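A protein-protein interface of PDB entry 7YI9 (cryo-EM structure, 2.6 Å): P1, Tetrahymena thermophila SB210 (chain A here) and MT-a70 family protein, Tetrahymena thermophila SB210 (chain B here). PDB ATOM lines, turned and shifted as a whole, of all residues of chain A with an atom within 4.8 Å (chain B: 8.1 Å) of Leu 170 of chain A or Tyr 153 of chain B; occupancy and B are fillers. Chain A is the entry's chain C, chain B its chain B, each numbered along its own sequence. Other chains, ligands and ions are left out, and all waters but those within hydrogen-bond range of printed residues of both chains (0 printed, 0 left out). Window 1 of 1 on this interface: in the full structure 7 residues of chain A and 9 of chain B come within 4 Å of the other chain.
Of chain A, only Glu 157 and Leu 170 come within 4 Å of Tyr 153 of chain B.
Printed residues of chain A within 4 Å of Ile 146 of chain B: Leu 170 (3.7 Å).
Of the printed residues of chain A, Ile 150 of chain B touches Leu 170 and Lys 174.
Of the printed residues of chain B, Glu 157 of chain A touches Tyr 153.
The nearest residue of chain B that does not touch Leu 170 of chain A is Arg 149 of chain B (5.0 Å).
Of the 17 printed residues of chain B, 3 touch a printed residue of chain A.
Hydrophobic or aromatic side chains of chain B that line the printed part of chain A: Ile 146, Ile 150 and Tyr 153.
Of the 10 printed residues of chain A, 3 touch a printed residue of chain B.
CG of Glu 157 of chain A touches OH of Tyr 153 of chain B (3.1 Å).
Ile 146 of chain B touches Leu 170 of chain A (CG2 to CD2, 3.7 Å).
Ile 150 of chain B touches Leu 170 of chain A.
Leu 170 of chain A touches Tyr 153 of chain B (CD1 to CD2, 3.98 Å).
Lys 174 of chain A touches Ile 150 of chain B (NZ to CG2, 3.6 Å).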
ATOM      1  N   GLU A 157      -5.458  -0.903  20.473  1.00  0.00           N
ATOM      2  CA  GLU A 157      -6.671  -1.359  19.806  1.00  0.00           C
ATOM      3  C   GLU A 157      -7.428  -2.429  20.583  1.00  0.00           C
ATOM      4  O   GLU A 157      -8.479  -2.881  20.120  1.00  0.00           O
ATOM      5  CB  GLU A 157      -6.332  -1.876  18.407  1.00  0.00           C
ATOM      6  CG  GLU A 157      -5.531  -3.165  18.400  1.00  0.00           C
ATOM      7  CD  GLU A 157      -4.037  -2.925  18.537  1.00  0.00           C
ATOM      8  OE1 GLU A 157      -3.639  -1.808  18.931  1.00  0.00           O
ATOM      9  OE2 GLU A 157      -3.256  -3.854  18.241  1.00  0.00           O
ATOM     10  N   ILE A 166     -10.332   4.459  16.553  1.00  0.00           N
ATOM     11  CA  ILE A 166      -9.477   3.273  16.644  1.00  0.00           C
ATOM     12  C   ILE A 166      -8.005   3.629  16.499  1.00  0.00           C
ATOM     13  O   ILE A 166      -7.131   2.878  16.947  1.00  0.00           O
ATOM     14  CB  ILE A 166      -9.902   2.223  15.599  1.00  0.00           C
ATOM     15  CG1 ILE A 166      -9.929   2.835  14.195  1.00  0.00           C
ATOM     16  CG2 ILE A 166     -11.249   1.622  15.961  1.00  0.00           C
ATOM     17  CD1 ILE A 166     -10.323   1.855  13.104  1.00  0.00           C
ATOM     18  N   LEU A 167      -7.700   4.759  15.871  1.00  0.00           N
ATOM     19  CA  LEU A 167      -6.334   5.275  15.836  1.00  0.00           C
ATOM     20  C   LEU A 167      -6.086   6.214  17.017  1.00  0.00           C
ATOM     21  O   LEU A 167      -5.646   7.348  16.851  1.00  0.00           O
ATOM     22  CB  LEU A 167      -6.074   5.987  14.511  1.00  0.00           C
ATOM     23  CG  LEU A 167      -5.844   5.209  13.210  1.00  0.00           C
ATOM     24  CD1 LEU A 167      -7.132   4.590  12.690  1.00  0.00           C
ATOM     25  CD2 LEU A 167      -5.224   6.101  12.147  1.00  0.00           C
ATOM     26  N   THR A 168      -6.362   5.734  18.235  1.00  0.00           N
ATOM     27  CA  THR A 168      -6.362   6.610  19.404  1.00  0.00           C
ATOM     28  C   THR A 168      -4.981   7.156  19.737  1.00  0.00           C
ATOM     29  O   THR A 168      -4.879   8.116  20.507  1.00  0.00           O
ATOM     30  CB  THR A 168      -6.921   5.876  20.623  1.00  0.00           C
ATOM     31  OG1 THR A 168      -7.133   6.812  21.688  1.00  0.00           O
ATOM     32  CG2 THR A 168      -5.954   4.805  21.090  1.00  0.00           C
ATOM     33  N   HIS A 169      -3.922   6.564  19.191  1.00  0.00           N
ATOM     34  CA  HIS A 169      -2.591   7.140  19.276  1.00  0.00           C
ATOM     35  C   HIS A 169      -1.880   7.211  17.938  1.00  0.00           C
ATOM     36  O   HIS A 169      -0.918   7.976  17.815  1.00  0.00           O
ATOM     37  CB  HIS A 169      -1.720   6.359  20.273  1.00  0.00           C
ATOM     38  CG  HIS A 169      -2.012   6.679  21.706  1.00  0.00           C
ATOM     39  ND1 HIS A 169      -2.792   7.751  22.082  1.00  0.00           N
ATOM     40  CD2 HIS A 169      -1.625   6.075  22.854  1.00  0.00           C
ATOM     41  CE1 HIS A 169      -2.878   7.789  23.400  1.00  0.00           C
ATOM     42  NE2 HIS A 169      -2.178   6.783  23.892  1.00  0.00           N
ATOM     43  N   LEU A 170      -2.332   6.457  16.932  1.00  0.00           N
ATOM     44  CA  LEU A 170      -1.789   6.610  15.588  1.00  0.00           C
ATOM     45  C   LEU A 170      -1.996   8.024  15.062  1.00  0.00           C
ATOM     46  O   LEU A 170      -1.251   8.458  14.175  1.00  0.00           O
ATOM     47  CB  LEU A 170      -2.424   5.582  14.648  1.00  0.00           C
ATOM     48  CG  LEU A 170      -2.080   4.117  14.946  1.00  0.00           C
ATOM     49  CD1 LEU A 170      -3.008   3.155  14.216  1.00  0.00           C
ATOM     50  CD2 LEU A 170      -0.629   3.814  14.610  1.00  0.00           C
ATOM     51  N   TYR A 171      -2.967   8.757  15.621  1.00  0.00           N
ATOM     52  CA  TYR A 171      -3.074  10.189  15.365  1.00  0.00           C
ATOM     53  C   TYR A 171      -1.750  10.888  15.638  1.00  0.00           C
ATOM     54  O   TYR A 171      -1.232  11.623  14.790  1.00  0.00           O
ATOM     55  CB  TYR A 171      -4.162  10.804  16.248  1.00  0.00           C
ATOM     56  CG  TYR A 171      -5.557  10.268  16.055  1.00  0.00           C
ATOM     57  CD1 TYR A 171      -5.930   9.630  14.883  1.00  0.00           C
ATOM     58  CD2 TYR A 171      -6.510  10.406  17.055  1.00  0.00           C
ATOM     59  CE1 TYR A 171      -7.214   9.148  14.713  1.00  0.00           C
ATOM     60  CE2 TYR A 171      -7.790   9.925  16.895  1.00  0.00           C
ATOM     61  CZ  TYR A 171      -8.135   9.296  15.724  1.00  0.00           C
ATOM     62  OH  TYR A 171      -9.409   8.816  15.560  1.00  0.00           O
ATOM     63  N   ASN A 172      -1.187  10.667  16.827  1.00  0.00           N
ATOM     64  CA  ASN A 172       0.081  11.279  17.193  1.00  0.00           C
ATOM     65  C   ASN A 172       1.279  10.415  16.834  1.00  0.00           C
ATOM     66  O   ASN A 172       2.380  10.949  16.669  1.00  0.00           O
ATOM     67  CB  ASN A 172       0.103  11.596  18.691  1.00  0.00           C
ATOM     68  CG  ASN A 172      -0.235  13.046  18.982  1.00  0.00           C
ATOM     69  OD1 ASN A 172      -0.040  13.921  18.139  1.00  0.00           O
ATOM     70  ND2 ASN A 172      -0.746  13.308  20.180  1.00  0.00           N
ATOM     71  N   LEU A 173       1.097   9.099  16.702  1.00  0.00           N
ATOM     72  CA  LEU A 173       2.170   8.275  16.161  1.00  0.00           C
ATOM     73  C   LEU A 173       2.502   8.660  14.726  1.00  0.00           C
ATOM     74  O   LEU A 173       3.633   8.431  14.279  1.00  0.00           O
ATOM     75  CB  LEU A 173       1.800   6.794  16.247  1.00  0.00           C
ATOM     76  CG  LEU A 173       1.679   6.233  17.665  1.00  0.00           C
ATOM     77  CD1 LEU A 173       1.173   4.799  17.654  1.00  0.00           C
ATOM     78  CD2 LEU A 173       3.013   6.326  18.387  1.00  0.00           C
ATOM     79  N   LYS A 174       1.550   9.270  14.011  1.00  0.00           N
ATOM     80  CA  LYS A 174       1.822   9.784  12.674  1.00  0.00           C
ATOM     81  C   LYS A 174       2.946  10.813  12.683  1.00  0.00           C
ATOM     82  O   LYS A 174       3.701  10.917  11.710  1.00  0.00           O
ATOM     83  CB  LYS A 174       0.548  10.392  12.087  1.00  0.00           C
ATOM     84  CG  LYS A 174       0.624  10.710  10.605  1.00  0.00           C
ATOM     85  CD  LYS A 174       0.488   9.450   9.768  1.00  0.00           C
ATOM     86  CE  LYS A 174      -0.941   8.937   9.788  1.00  0.00           C
ATOM     87  NZ  LYS A 174      -1.147   7.819   8.827  1.00  0.00           N
ATOM     88  N   ASP B 145       6.105  -1.691  10.909  1.00  0.00           N
ATOM     89  CA  ASP B 145       4.941  -2.364  11.478  1.00  0.00           C
ATOM     90  C   ASP B 145       3.812  -1.379  11.752  1.00  0.00           C
ATOM     91  O   ASP B 145       2.637  -1.684  11.507  1.00  0.00           O
ATOM     92  CB  ASP B 145       5.329  -3.109  12.755  1.00  0.00           C
ATOM     93  CG  ASP B 145       5.825  -4.514  12.480  1.00  0.00           C
ATOM     94  OD1 ASP B 145       5.402  -5.103  11.463  1.00  0.00           O
ATOM     95  OD2 ASP B 145       6.629  -5.033  13.282  1.00  0.00           O
ATOM     96  N   ILE B 146       4.146  -0.190  12.260  1.00  0.00           N
ATOM     97  CA  ILE B 146       3.131   0.827  12.506  1.00  0.00           C
ATOM     98  C   ILE B 146       2.480   1.257  11.200  1.00  0.00           C
ATOM     99  O   ILE B 146       1.264   1.450  11.136  1.00  0.00           O
ATOM    100  CB  ILE B 146       3.739   2.023  13.264  1.00  0.00           C
ATOM    101  CG1 ILE B 146       4.090   1.619  14.697  1.00  0.00           C
ATOM    102  CG2 ILE B 146       2.780   3.201  13.271  1.00  0.00           C
ATOM    103  CD1 ILE B 146       4.917   2.646  15.436  1.00  0.00           C
ATOM    104  N   GLU B 147       3.275   1.405  10.136  1.00  0.00           N
ATOM    105  CA  GLU B 147       2.712   1.789   8.845  1.00  0.00           C
ATOM    106  C   GLU B 147       1.774   0.715   8.303  1.00  0.00           C
ATOM    107  O   GLU B 147       0.706   1.026   7.762  1.00  0.00           O
ATOM    108  CB  GLU B 147       3.835   2.076   7.849  1.00  0.00           C
ATOM    109  CG  GLU B 147       3.353   2.488   6.468  1.00  0.00           C
ATOM    110  CD  GLU B 147       2.648   3.833   6.469  1.00  0.00           C
ATOM    111  OE1 GLU B 147       2.952   4.667   7.347  1.00  0.00           O
ATOM    112  OE2 GLU B 147       1.789   4.054   5.591  1.00  0.00           O
ATOM    113  N   LYS B 148       2.159  -0.557   8.435  1.00  0.00           N
ATOM    114  CA  LYS B 148       1.289  -1.634   7.968  1.00  0.00           C
ATOM    115  C   LYS B 148      -0.009  -1.687   8.769  1.00  0.00           C
ATOM    116  O   LYS B 148      -1.097  -1.858   8.199  1.00  0.00           O
ATOM    117  CB  LYS B 148       2.027  -2.970   8.038  1.00  0.00           C
ATOM    118  CG  LYS B 148       3.073  -3.148   6.946  1.00  0.00           C
ATOM    119  CD  LYS B 148       3.640  -4.556   6.938  1.00  0.00           C
ATOM    120  CE  LYS B 148       4.588  -4.759   5.767  1.00  0.00           C
ATOM    121  NZ  LYS B 148       5.148  -6.137   5.739  1.00  0.00           N
ATOM    122  N   ARG B 149       0.085  -1.537  10.092  1.00  0.00           N
ATOM    123  CA  ARG B 149      -1.117  -1.500  10.917  1.00  0.00           C
ATOM    124  C   ARG B 149      -1.984  -0.296  10.567  1.00  0.00           C
ATOM    125  O   ARG B 149      -3.219  -0.379  10.586  1.00  0.00           O
ATOM    126  CB  ARG B 149      -0.733  -1.478  12.396  1.00  0.00           C
ATOM    127  CG  ARG B 149      -1.909  -1.603  13.344  1.00  0.00           C
ATOM    128  CD  ARG B 149      -2.170  -3.052  13.726  1.00  0.00           C
ATOM    129  NE  ARG B 149      -2.932  -3.755  12.701  1.00  0.00           N
ATOM    130  CZ  ARG B 149      -3.266  -5.036  12.764  1.00  0.00           C
ATOM    131  NH1 ARG B 149      -2.939  -5.784  13.804  1.00  0.00           N
ATOM    132  NH2 ARG B 149      -3.947  -5.578  11.760  1.00  0.00           N
ATOM    133  N   ILE B 150      -1.348   0.834  10.251  1.00  0.00           N
ATOM    134  CA  ILE B 150      -2.073   2.025   9.825  1.00  0.00           C
ATOM    135  C   ILE B 150      -2.842   1.743   8.546  1.00  0.00           C
ATOM    136  O   ILE B 150      -4.006   2.126   8.414  1.00  0.00           O
ATOM    137  CB  ILE B 150      -1.099   3.207   9.650  1.00  0.00           C
ATOM    138  CG1 ILE B 150      -0.774   3.842  11.002  1.00  0.00           C
ATOM    139  CG2 ILE B 150      -1.670   4.244   8.694  1.00  0.00           C
ATOM    140  CD1 ILE B 150       0.356   4.851  10.944  1.00  0.00           C
ATOM    141  N   LEU B 151      -2.205   1.070   7.586  1.00  0.00           N
ATOM    142  CA  LEU B 151      -2.890   0.728   6.343  1.00  0.00           C
ATOM    143  C   LEU B 151      -4.074  -0.200   6.599  1.00  0.00           C
ATOM    144  O   LEU B 151      -5.155  -0.018   6.023  1.00  0.00           O
ATOM    145  CB  LEU B 151      -1.907   0.089   5.363  1.00  0.00           C
ATOM    146  CG  LEU B 151      -2.303   0.109   3.886  1.00  0.00           C
ATOM    147  CD1 LEU B 151      -2.686   1.512   3.449  1.00  0.00           C
ATOM    148  CD2 LEU B 151      -1.171  -0.431   3.028  1.00  0.00           C
ATOM    149  N   HIS B 152      -3.887  -1.197   7.466  1.00  0.00           N
ATOM    150  CA  HIS B 152      -4.973  -2.125   7.776  1.00  0.00           C
ATOM    151  C   HIS B 152      -6.159  -1.399   8.405  1.00  0.00           C
ATOM    152  O   HIS B 152      -7.310  -1.549   7.964  1.00  0.00           O
ATOM    153  CB  HIS B 152      -4.459  -3.228   8.702  1.00  0.00           C
ATOM    154  CG  HIS B 152      -5.477  -4.275   9.026  1.00  0.00           C
ATOM    155  ND1 HIS B 152      -6.171  -4.295  10.218  1.00  0.00           N
ATOM    156  CD2 HIS B 152      -5.914  -5.343   8.319  1.00  0.00           C
ATOM    157  CE1 HIS B 152      -6.994  -5.327  10.229  1.00  0.00           C
ATOM    158  NE2 HIS B 152      -6.858  -5.980   9.089  1.00  0.00           N
ATOM    159  N   TYR B 153      -5.896  -0.595   9.439  1.00  0.00           N
ATOM    160  CA  TYR B 153      -6.977   0.125  10.102  1.00  0.00           C
ATOM    161  C   TYR B 153      -7.584   1.189   9.199  1.00  0.00           C
ATOM    162  O   TYR B 153      -8.774   1.484   9.318  1.00  0.00           O
ATOM    163  CB  TYR B 153      -6.480   0.741  11.408  1.00  0.00           C
ATOM    164  CG  TYR B 153      -6.146  -0.290  12.461  1.00  0.00           C
ATOM    165  CD1 TYR B 153      -6.578  -1.602  12.329  1.00  0.00           C
ATOM    166  CD2 TYR B 153      -5.398   0.043  13.579  1.00  0.00           C
ATOM    167  CE1 TYR B 153      -6.278  -2.552  13.279  1.00  0.00           C
ATOM    168  CE2 TYR B 153      -5.093  -0.902  14.536  1.00  0.00           C
ATOM    169  CZ  TYR B 153      -5.535  -2.197  14.379  1.00  0.00           C
ATOM    170  OH  TYR B 153      -5.235  -3.147  15.325  1.00  0.00           O
ATOM    171  N   LYS B 154      -6.795   1.758   8.286  1.00  0.00           N
ATOM    172  CA  LYS B 154      -7.347   2.670   7.293  1.00  0.00           C
ATOM    173  C   LYS B 154      -8.333   1.958   6.385  1.00  0.00           C
ATOM    174  O   LYS B 154      -9.397   2.498   6.075  1.00  0.00           O
ATOM    175  CB  LYS B 154      -6.221   3.291   6.468  1.00  0.00           C
ATOM    176  CG  LYS B 154      -5.590   4.528   7.082  1.00  0.00           C
ATOM    177  CD  LYS B 154      -4.381   4.971   6.277  1.00  0.00           C
ATOM    178  CE  LYS B 154      -4.774   5.354   4.861  1.00  0.00           C
ATOM    179  NZ  LYS B 154      -3.619   5.897   4.097  1.00  0.00           N
ATOM    180  N   GLN B 155      -7.996   0.745   5.942  1.00  0.00           N
ATOM    181  CA  GLN B 155      -8.919  -0.004   5.096  1.00  0.00           C
ATOM    182  C   GLN B 155     -10.203  -0.333   5.852  1.00  0.00           C
ATOM    183  O   GLN B 155     -11.307  -0.220   5.305  1.00  0.00           O
ATOM    184  CB  GLN B 155      -8.246  -1.274   4.578  1.00  0.00           C
ATOM    185  CG  GLN B 155      -8.948  -1.901   3.386  1.00  0.00           C
ATOM    186  CD  GLN B 155      -8.146  -3.027   2.761  1.00  0.00           C
ATOM    187  OE1 GLN B 155      -7.080  -3.395   3.255  1.00  0.00           O
ATOM    188  NE2 GLN B 155      -8.657  -3.579   1.666  1.00  0.00           N
ATOM    189  N   LEU B 156     -10.076  -0.731   7.122  1.00  0.00           N
ATOM    190  CA  LEU B 156     -11.273  -0.990   7.924  1.00  0.00           C
ATOM    191  C   LEU B 156     -12.115   0.274   8.100  1.00  0.00           C
ATOM    192  O   LEU B 156     -13.347   0.233   7.978  1.00  0.00           O
ATOM    193  CB  LEU B 156     -10.888  -1.574   9.283  1.00  0.00           C
ATOM    194  CG  LEU B 156     -10.826  -3.102   9.379  1.00  0.00           C
ATOM    195  CD1 LEU B 156      -9.623  -3.664   8.644  1.00  0.00           C
ATOM    196  CD2 LEU B 156     -10.822  -3.545  10.833  1.00  0.00           C
ATOM    197  N   PHE B 157     -11.462   1.404   8.383  1.00  0.00           N
ATOM    198  CA  PHE B 157     -12.134   2.694   8.488  1.00  0.00           C
ATOM    199  C   PHE B 157     -12.922   3.004   7.222  1.00  0.00           C
ATOM    200  O   PHE B 157     -14.117   3.322   7.268  1.00  0.00           O
ATOM    201  CB  PHE B 157     -11.075   3.774   8.748  1.00  0.00           C
ATOM    202  CG  PHE B 157     -11.624   5.167   8.908  1.00  0.00           C
ATOM    203  CD1 PHE B 157     -12.172   5.580  10.108  1.00  0.00           C
ATOM    204  CD2 PHE B 157     -11.571   6.069   7.859  1.00  0.00           C
ATOM    205  CE1 PHE B 157     -12.662   6.863  10.254  1.00  0.00           C
ATOM    206  CE2 PHE B 157     -12.065   7.351   7.999  1.00  0.00           C
ATOM    207  CZ  PHE B 157     -12.612   7.746   9.196  1.00  0.00           C
ATOM    208  N   PHE B 158     -12.249   2.905   6.076  1.00  0.00           N
ATOM    209  CA  PHE B 158     -12.863   3.256   4.802  1.00  0.00           C
ATOM    210  C   PHE B 158     -14.039   2.344   4.494  1.00  0.00           C
ATOM    211  O   PHE B 158     -15.081   2.804   4.010  1.00  0.00           O
ATOM    212  CB  PHE B 158     -11.817   3.201   3.689  1.00  0.00           C
ATOM    213  CG  PHE B 158     -10.776   4.295   3.763  1.00  0.00           C
ATOM    214  CD1 PHE B 158     -10.511   4.960   4.948  1.00  0.00           C
ATOM    215  CD2 PHE B 158     -10.027   4.619   2.654  1.00  0.00           C
ATOM    216  CE1 PHE B 158      -9.550   5.946   5.012  1.00  0.00           C
ATOM    217  CE2 PHE B 158      -9.060   5.603   2.714  1.00  0.00           C
ATOM    218  CZ  PHE B 158      -8.824   6.267   3.893  1.00  0.00           C
ATOM    219  N   LYS B 159     -13.902   1.046   4.786  1.00  0.00           N
ATOM    220  CA  LYS B 159     -15.027   0.133   4.610  1.00  0.00           C
ATOM    221  C   LYS B 159     -16.199   0.526   5.499  1.00  0.00           C
ATOM    222  O   LYS B 159     -17.357   0.474   5.070  1.00  0.00           O
ATOM    223  CB  LYS B 159     -14.592  -1.303   4.901  1.00  0.00           C
ATOM    224  CG  LYS B 159     -15.572  -2.361   4.412  1.00  0.00           C
ATOM    225  CD  LYS B 159     -16.497  -2.820   5.528  1.00  0.00           C
ATOM    226  CE  LYS B 159     -17.509  -3.834   5.027  1.00  0.00           C
ATOM    227  NZ  LYS B 159     -18.443  -4.254   6.106  1.00  0.00           N
ATOM    228  N   GLU B 160     -15.920   0.917   6.743  1.00  0.00           N
ATOM    229  CA  GLU B 160     -17.001   1.265   7.661  1.00  0.00           C
ATOM    230  C   GLU B 160     -17.756   2.510   7.204  1.00  0.00           C
ATOM    231  O   GLU B 160     -18.991   2.519   7.195  1.00  0.00           O
ATOM    232  CB  GLU B 160     -16.455   1.444   9.072  1.00  0.00           C
ATOM    233  CG  GLU B 160     -17.518   1.770  10.112  1.00  0.00           C
ATOM    234  CD  GLU B 160     -18.513   0.646  10.321  1.00  0.00           C
ATOM    235  OE1 GLU B 160     -18.161  -0.525  10.071  1.00  0.00           O
ATOM    236  OE2 GLU B 160     -19.648   0.937  10.750  1.00  0.00           O
ATOM    237  N   GLN B 161     -17.043   3.581   6.831  1.00  0.00           N
ATOM    238  CA  GLN B 161     -17.782   4.737   6.313  1.00  0.00           C
ATOM    239  C   GLN B 161     -18.426   4.478   4.953  1.00  0.00           C
ATOM    240  O   GLN B 161     -19.468   5.073   4.662  1.00  0.00           O
ATOM    241  CB  GLN B 161     -16.954   6.032   6.265  1.00  0.00           C
ATOM    242  CG  GLN B 161     -16.745   6.742   7.617  1.00  0.00           C
ATOM    243  CD  GLN B 161     -15.604   6.252   8.463  1.00  0.00           C
ATOM    244  OE1 GLN B 161     -14.690   5.608   7.978  1.00  0.00           O
ATOM    245  NE2 GLN B 161     -15.662   6.555   9.754  1.00  0.00           N
